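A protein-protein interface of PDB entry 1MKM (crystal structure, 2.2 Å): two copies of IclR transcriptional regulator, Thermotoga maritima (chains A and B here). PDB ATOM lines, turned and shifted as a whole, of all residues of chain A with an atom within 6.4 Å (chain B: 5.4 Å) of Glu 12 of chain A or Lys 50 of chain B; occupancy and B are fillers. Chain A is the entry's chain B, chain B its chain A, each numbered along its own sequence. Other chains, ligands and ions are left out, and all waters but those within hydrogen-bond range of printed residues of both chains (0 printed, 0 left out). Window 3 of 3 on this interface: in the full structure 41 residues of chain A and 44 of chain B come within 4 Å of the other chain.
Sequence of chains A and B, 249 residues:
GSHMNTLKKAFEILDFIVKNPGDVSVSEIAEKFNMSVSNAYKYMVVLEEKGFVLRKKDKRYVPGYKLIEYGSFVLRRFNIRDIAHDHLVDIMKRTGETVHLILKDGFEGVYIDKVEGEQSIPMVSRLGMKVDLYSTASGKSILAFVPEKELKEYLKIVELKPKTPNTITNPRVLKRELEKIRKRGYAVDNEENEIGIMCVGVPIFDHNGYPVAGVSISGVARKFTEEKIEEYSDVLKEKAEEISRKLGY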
ATOM      1  N   LEU A   7     -16.918  -3.103  20.168  1.00  0.00           N
ATOM      2  CA  LEU A   7     -17.275  -4.497  19.981  1.00  0.00           C
ATOM      3  C   LEU A   7     -17.117  -5.212  21.297  1.00  0.00           C
ATOM      4  O   LEU A   7     -17.986  -5.983  21.693  1.00  0.00           O
ATOM      5  CB  LEU A   7     -16.348  -5.150  18.954  1.00  0.00           C
ATOM      6  CG  LEU A   7     -16.380  -4.570  17.546  1.00  0.00           C
ATOM      7  CD1 LEU A   7     -15.283  -5.193  16.712  1.00  0.00           C
ATOM      8  CD2 LEU A   7     -17.742  -4.826  16.926  1.00  0.00           C
ATOM      9  N   LYS A   8     -15.997  -4.964  21.971  1.00  0.00           N
ATOM     10  CA  LYS A   8     -15.759  -5.590  23.264  1.00  0.00           C
ATOM     11  C   LYS A   8     -16.909  -5.294  24.217  1.00  0.00           C
ATOM     12  O   LYS A   8     -17.511  -6.212  24.777  1.00  0.00           O
ATOM     13  CB  LYS A   8     -14.456  -5.092  23.884  1.00  0.00           C
ATOM     14  CG  LYS A   8     -13.222  -5.772  23.348  1.00  0.00           C
ATOM     15  CD  LYS A   8     -12.058  -5.586  24.300  1.00  0.00           C
ATOM     16  CE  LYS A   8     -10.796  -6.200  23.735  1.00  0.00           C
ATOM     17  NZ  LYS A   8     -10.433  -5.594  22.415  1.00  0.00           N
ATOM     18  N   LYS A   9     -17.217  -4.013  24.389  1.00  0.00           N
ATOM     19  CA  LYS A   9     -18.288  -3.607  25.290  1.00  0.00           C
ATOM     20  C   LYS A   9     -19.584  -4.350  24.986  1.00  0.00           C
ATOM     21  O   LYS A   9     -20.276  -4.818  25.893  1.00  0.00           O
ATOM     22  CB  LYS A   9     -18.533  -2.099  25.190  1.00  0.00           C
ATOM     23  CG  LYS A   9     -19.625  -1.605  26.124  1.00  0.00           C
ATOM     24  CD  LYS A   9     -19.277  -1.908  27.570  1.00  0.00           C
ATOM     25  CE  LYS A   9     -18.104  -1.061  28.043  1.00  0.00           C
ATOM     26  NZ  LYS A   9     -18.435   0.394  28.025  1.00  0.00           N
ATOM     27  N   ALA A  10     -19.906  -4.444  23.701  1.00  0.00           N
ATOM     28  CA  ALA A  10     -21.110  -5.124  23.260  1.00  0.00           C
ATOM     29  C   ALA A  10     -21.138  -6.547  23.815  1.00  0.00           C
ATOM     30  O   ALA A  10     -22.103  -6.954  24.461  1.00  0.00           O
ATOM     31  CB  ALA A  10     -21.159  -5.153  21.737  1.00  0.00           C
ATOM     32  N   PHE A  11     -20.060  -7.287  23.570  1.00  0.00           N
ATOM     33  CA  PHE A  11     -19.955  -8.669  24.021  1.00  0.00           C
ATOM     34  C   PHE A  11     -19.794  -8.867  25.520  1.00  0.00           C
ATOM     35  O   PHE A  11     -19.872  -9.988  26.010  1.00  0.00           O
ATOM     36  CB  PHE A  11     -18.835  -9.368  23.257  1.00  0.00           C
ATOM     37  CG  PHE A  11     -19.183  -9.628  21.827  1.00  0.00           C
ATOM     38  CD1 PHE A  11     -20.137 -10.587  21.501  1.00  0.00           C
ATOM     39  CD2 PHE A  11     -18.616  -8.872  20.808  1.00  0.00           C
ATOM     40  CE1 PHE A  11     -20.524 -10.786  20.186  1.00  0.00           C
ATOM     41  CE2 PHE A  11     -18.994  -9.057  19.491  1.00  0.00           C
ATOM     42  CZ  PHE A  11     -19.953 -10.020  19.176  1.00  0.00           C
ATOM     43  N   GLU A  12     -19.561  -7.783  26.247  1.00  0.00           N
ATOM     44  CA  GLU A  12     -19.448  -7.866  27.691  1.00  0.00           C
ATOM     45  C   GLU A  12     -20.857  -7.688  28.242  1.00  0.00           C
ATOM     46  O   GLU A  12     -21.262  -8.366  29.185  1.00  0.00           O
ATOM     47  CB  GLU A  12     -18.511  -6.781  28.225  1.00  0.00           C
ATOM     48  CG  GLU A  12     -17.048  -7.202  28.217  1.00  0.00           C
ATOM     49  CD  GLU A  12     -16.092  -6.052  28.487  1.00  0.00           C
ATOM     50  OE1 GLU A  12     -16.285  -5.321  29.484  1.00  0.00           O
ATOM     51  OE2 GLU A  12     -15.135  -5.887  27.695  1.00  0.00           O
ATOM     52  N   ILE A  13     -21.608  -6.775  27.636  1.00  0.00           N
ATOM     53  CA  ILE A  13     -22.979  -6.543  28.067  1.00  0.00           C
ATOM     54  C   ILE A  13     -23.803  -7.813  27.809  1.00  0.00           C
ATOM     55  O   ILE A  13     -24.529  -8.282  28.683  1.00  0.00           O
ATOM     56  CB  ILE A  13     -23.608  -5.367  27.304  1.00  0.00           C
ATOM     57  CG1 ILE A  13     -22.790  -4.103  27.556  1.00  0.00           C
ATOM     58  CG2 ILE A  13     -25.057  -5.182  27.729  1.00  0.00           C
ATOM     59  CD1 ILE A  13     -23.429  -2.870  27.020  1.00  0.00           C
ATOM     60  N   LEU A  14     -23.672  -8.361  26.604  1.00  0.00           N
ATOM     61  CA  LEU A  14     -24.396  -9.567  26.232  1.00  0.00           C
ATOM     62  C   LEU A  14     -24.006 -10.732  27.138  1.00  0.00           C
ATOM     63  O   LEU A  14     -24.878 -11.403  27.686  1.00  0.00           O
ATOM     64  CB  LEU A  14     -24.125  -9.921  24.767  1.00  0.00           C
ATOM     65  CG  LEU A  14     -24.705 -11.233  24.207  1.00  0.00           C
ATOM     66  CD1 LEU A  14     -26.222 -11.203  24.232  1.00  0.00           C
ATOM     67  CD2 LEU A  14     -24.211 -11.441  22.767  1.00  0.00           C
ATOM     68  N   ASP A  15     -22.705 -10.969  27.307  1.00  0.00           N
ATOM     69  CA  ASP A  15     -22.256 -12.065  28.158  1.00  0.00           C
ATOM     70  C   ASP A  15     -22.900 -11.959  29.522  1.00  0.00           C
ATOM     71  O   ASP A  15     -23.215 -12.973  30.151  1.00  0.00           O
ATOM     72  CB  ASP A  15     -20.734 -12.067  28.313  1.00  0.00           C
ATOM     73  CG  ASP A  15     -20.243 -13.160  29.261  1.00  0.00           C
ATOM     74  OD1 ASP A  15     -20.221 -12.935  30.490  1.00  0.00           O
ATOM     75  OD2 ASP A  15     -19.891 -14.258  28.782  1.00  0.00           O
ATOM     76  N   PHE A  16     -23.113 -10.722  29.963  1.00  0.00           N
ATOM     77  CA  PHE A  16     -23.717 -10.449  31.261  1.00  0.00           C
ATOM     78  C   PHE A  16     -25.206 -10.788  31.347  1.00  0.00           C
ATOM     79  O   PHE A  16     -25.663 -11.320  32.352  1.00  0.00           O
ATOM     80  CB  PHE A  16     -23.516  -8.975  31.634  1.00  0.00           C
ATOM     81  CG  PHE A  16     -24.348  -8.528  32.808  1.00  0.00           C
ATOM     82  CD1 PHE A  16     -24.102  -9.027  34.087  1.00  0.00           C
ATOM     83  CD2 PHE A  16     -25.396  -7.626  32.627  1.00  0.00           C
ATOM     84  CE1 PHE A  16     -24.884  -8.642  35.173  1.00  0.00           C
ATOM     85  CE2 PHE A  16     -26.191  -7.228  33.698  1.00  0.00           C
ATOM     86  CZ  PHE A  16     -25.934  -7.740  34.982  1.00  0.00           C
ATOM     87  N   ILE A  17     -25.967 -10.465  30.313  1.00  0.00           N
ATOM     88  CA  ILE A  17     -27.395 -10.742  30.345  1.00  0.00           C
ATOM     89  C   ILE A  17     -27.637 -12.245  30.307  1.00  0.00           C
ATOM     90  O   ILE A  17     -28.595 -12.742  30.907  1.00  0.00           O
ATOM     91  CB  ILE A  17     -28.120 -10.037  29.168  1.00  0.00           C
ATOM     92  CG1 ILE A  17     -27.855  -8.525  29.247  1.00  0.00           C
ATOM     93  CG2 ILE A  17     -29.617 -10.325  29.213  1.00  0.00           C
ATOM     94  CD1 ILE A  17     -28.447  -7.743  28.115  1.00  0.00           C
ATOM     95  N   PHE A  33     -22.125  -0.522  33.067  1.00  0.00           N
ATOM     96  CA  PHE A  33     -20.973  -0.265  32.213  1.00  0.00           C
ATOM     97  C   PHE A  33     -20.702   1.210  31.955  1.00  0.00           C
ATOM     98  O   PHE A  33     -20.513   1.625  30.810  1.00  0.00           O
ATOM     99  CB  PHE A  33     -21.127  -0.994  30.875  1.00  0.00           C
ATOM    100  CG  PHE A  33     -21.233  -2.490  31.007  1.00  0.00           C
ATOM    101  CD1 PHE A  33     -22.458  -3.097  31.251  1.00  0.00           C
ATOM    102  CD2 PHE A  33     -20.098  -3.289  30.918  1.00  0.00           C
ATOM    103  CE1 PHE A  33     -22.553  -4.471  31.405  1.00  0.00           C
ATOM    104  CE2 PHE A  33     -20.181  -4.666  31.071  1.00  0.00           C
ATOM    105  CZ  PHE A  33     -21.414  -5.259  31.316  1.00  0.00           C
ATOM    106  N   VAL B  45     -10.600 -10.417  15.618  1.00  0.00           N
ATOM    107  CA  VAL B  45      -9.765 -10.563  16.793  1.00  0.00           C
ATOM    108  C   VAL B  45     -10.620 -10.645  18.050  1.00  0.00           C
ATOM    109  O   VAL B  45     -10.297 -11.390  18.978  1.00  0.00           O
ATOM    110  CB  VAL B  45      -8.781  -9.394  16.933  1.00  0.00           C
ATOM    111  CG1 VAL B  45      -9.533  -8.094  17.075  1.00  0.00           C
ATOM    112  CG2 VAL B  45      -7.894  -9.612  18.142  1.00  0.00           C
ATOM    113  N   VAL B  46     -11.710  -9.877  18.073  1.00  0.00           N
ATOM    114  CA  VAL B  46     -12.618  -9.843  19.216  1.00  0.00           C
ATOM    115  C   VAL B  46     -13.517 -11.102  19.267  1.00  0.00           C
ATOM    116  O   VAL B  46     -13.648 -11.729  20.315  1.00  0.00           O
ATOM    117  CB  VAL B  46     -13.469  -8.524  19.182  1.00  0.00           C
ATOM    118  CG1 VAL B  46     -14.431  -8.463  20.346  1.00  0.00           C
ATOM    119  CG2 VAL B  46     -12.533  -7.305  19.227  1.00  0.00           C
ATOM    120  N   LEU B  47     -14.118 -11.482  18.141  1.00  0.00           N
ATOM    121  CA  LEU B  47     -14.956 -12.668  18.106  1.00  0.00           C
ATOM    122  C   LEU B  47     -14.140 -13.879  18.545  1.00  0.00           C
ATOM    123  O   LEU B  47     -14.641 -14.742  19.273  1.00  0.00           O
ATOM    124  CB  LEU B  47     -15.515 -12.907  16.703  1.00  0.00           C
ATOM    125  CG  LEU B  47     -16.502 -11.850  16.190  1.00  0.00           C
ATOM    126  CD1 LEU B  47     -16.855 -12.171  14.744  1.00  0.00           C
ATOM    127  CD2 LEU B  47     -17.756 -11.822  17.061  1.00  0.00           C
ATOM    128  N   GLU B  48     -12.886 -13.957  18.110  1.00  0.00           N
ATOM    129  CA  GLU B  48     -12.062 -15.085  18.522  1.00  0.00           C
ATOM    130  C   GLU B  48     -11.799 -14.914  20.009  1.00  0.00           C
ATOM    131  O   GLU B  48     -11.866 -15.869  20.777  1.00  0.00           O
ATOM    132  CB  GLU B  48     -10.746 -15.133  17.736  1.00  0.00           C
ATOM    133  CG  GLU B  48      -9.805 -16.241  18.195  1.00  0.00           C
ATOM    134  CD  GLU B  48      -8.763 -16.624  17.153  1.00  0.00           C
ATOM    135  OE1 GLU B  48      -8.104 -15.724  16.601  1.00  0.00           O
ATOM    136  OE2 GLU B  48      -8.595 -17.836  16.892  1.00  0.00           O
ATOM    137  N   GLU B  49     -11.544 -13.676  20.413  1.00  0.00           N
ATOM    138  CA  GLU B  49     -11.285 -13.349  21.810  1.00  0.00           C
ATOM    139  C   GLU B  49     -12.357 -13.947  22.731  1.00  0.00           C
ATOM    140  O   GLU B  49     -12.054 -14.745  23.621  1.00  0.00           O
ATOM    141  CB  GLU B  49     -11.243 -11.823  21.971  1.00  0.00           C
ATOM    142  CG  GLU B  49     -11.254 -11.290  23.409  1.00  0.00           C
ATOM    143  CD  GLU B  49     -11.429  -9.765  23.470  1.00  0.00           C
ATOM    144  OE1 GLU B  49     -12.377  -9.242  22.845  1.00  0.00           O
ATOM    145  OE2 GLU B  49     -10.626  -9.089  24.147  1.00  0.00           O
ATOM    146  N   LYS B  50     -13.610 -13.562  22.499  1.00  0.00           N
ATOM    147  CA  LYS B  50     -14.731 -14.023  23.318  1.00  0.00           C
ATOM    148  C   LYS B  50     -15.104 -15.489  23.038  1.00  0.00           C
ATOM    149  O   LYS B  50     -16.048 -16.026  23.607  1.00  0.00           O
ATOM    150  CB  LYS B  50     -15.925 -13.098  23.096  1.00  0.00           C
ATOM    151  CG  LYS B  50     -15.606 -11.625  23.318  1.00  0.00           C
ATOM    152  CD  LYS B  50     -15.162 -11.373  24.740  1.00  0.00           C
ATOM    153  CE  LYS B  50     -14.802  -9.916  24.947  1.00  0.00           C
ATOM    154  NZ  LYS B  50     -14.582  -9.612  26.391  1.00  0.00           N
ATOM    155  N   GLY B  51     -14.347 -16.133  22.160  1.00  0.00           N
ATOM    156  CA  GLY B  51     -14.589 -17.535  21.883  1.00  0.00           C
ATOM    157  C   GLY B  51     -15.742 -17.863  20.969  1.00  0.00           C
ATOM    158  O   GLY B  51     -16.056 -19.026  20.829  1.00  0.00           O
ATOM    159  N   PHE B  52     -16.354 -16.858  20.351  1.00  0.00           N
ATOM    160  CA  PHE B  52     -17.477 -17.067  19.450  1.00  0.00           C
ATOM    161  C   PHE B  52     -16.973 -17.551  18.120  1.00  0.00           C
ATOM    162  O   PHE B  52     -17.761 -17.876  17.237  1.00  0.00           O
ATOM    163  CB  PHE B  52     -18.252 -15.770  19.208  1.00  0.00           C
ATOM    164  CG  PHE B  52     -18.943 -15.221  20.429  1.00  0.00           C
ATOM    165  CD1 PHE B  52     -18.217 -14.780  21.527  1.00  0.00           C
ATOM    166  CD2 PHE B  52     -20.321 -15.091  20.456  1.00  0.00           C
ATOM    167  CE1 PHE B  52     -18.859 -14.211  22.628  1.00  0.00           C
ATOM    168  CE2 PHE B  52     -20.965 -14.527  21.550  1.00  0.00           C
ATOM    169  CZ  PHE B  52     -20.228 -14.086  22.635  1.00  0.00           C
ATOM    170  N   LYS B  66     -18.130 -21.559  22.350  1.00  0.00           N
ATOM    171  CA  LYS B  66     -18.867 -20.678  23.243  1.00  0.00           C
ATOM    172  C   LYS B  66     -20.328 -20.522  22.816  1.00  0.00           C
ATOM    173  O   LYS B  66     -21.192 -20.364  23.654  1.00  0.00           O
ATOM    174  CB  LYS B  66     -18.203 -19.296  23.284  1.00  0.00           C
ATOM    175  CG  LYS B  66     -18.666 -18.419  24.431  1.00  0.00           C
ATOM    176  CD  LYS B  66     -18.254 -19.033  25.763  1.00  0.00           C
ATOM    177  CE  LYS B  66     -17.561 -18.010  26.645  1.00  0.00           C
ATOM    178  NZ  LYS B  66     -18.375 -16.760  26.808  1.00  0.00           N
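O of Leu 47 of chain B is in hydrogen-bond range of N of Phe 52 of chain B.
The side-chain amino group of Lys 66 of chain B is in salt-bridge range of the side-chain carboxylate of Asp 15 of chain A (3.5 Å). OE2 of Glu 12 of chain A lies within salt-bridge range of NZ of Lys 50 of chain B, 3.99 Å away. OE2 of Glu 49 of chain B lies within salt-bridge range of NZ of Lys 8 of chain A, 3.9 Å away.
Hydrophobic or aromatic side chains of chain A that line the printed part of chain B: Phe 11. Of the 9 printed residues of chain B, 5 touch a printed residue of chain A. Hydrophobic or aromatic side chains of chain B that line the printed part of chain A: Leu 47 and Phe 52.
Phe 11 of chain A touches Leu 47 of chain B. CB of Phe 11 of chain A touches CG of Lys 50 of chain B (3.9 Å). Phe 11 of chain A touches Phe 52 of chain B.
No position is printed for both chains. Of the 6 pairs that touch across the chains among the printed residues, none has its exchanged pair printed and touching as well.
Of the printed residues of chain B, Phe 11 of chain A touches Leu 47, Lys 50 and Phe 52. Of chain B, only Lys 50 (3.9 Å) comes within 4 Å of Glu 12 of chain A. Of the printed residues of chain B, Asp 15 of chain A touches Lys 66 (3.5 Å). Val 46 of chain B touches none of the printed residues of chain A. Lys 50 of chain B touches two residues of chain A. Of the printed residues of chain A, Phe 52 of chain B touches Phe 11. The nearest residue of chain A that does not touch Lys 50 of chain B is Lys 8 of chain A (4.6 Å).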
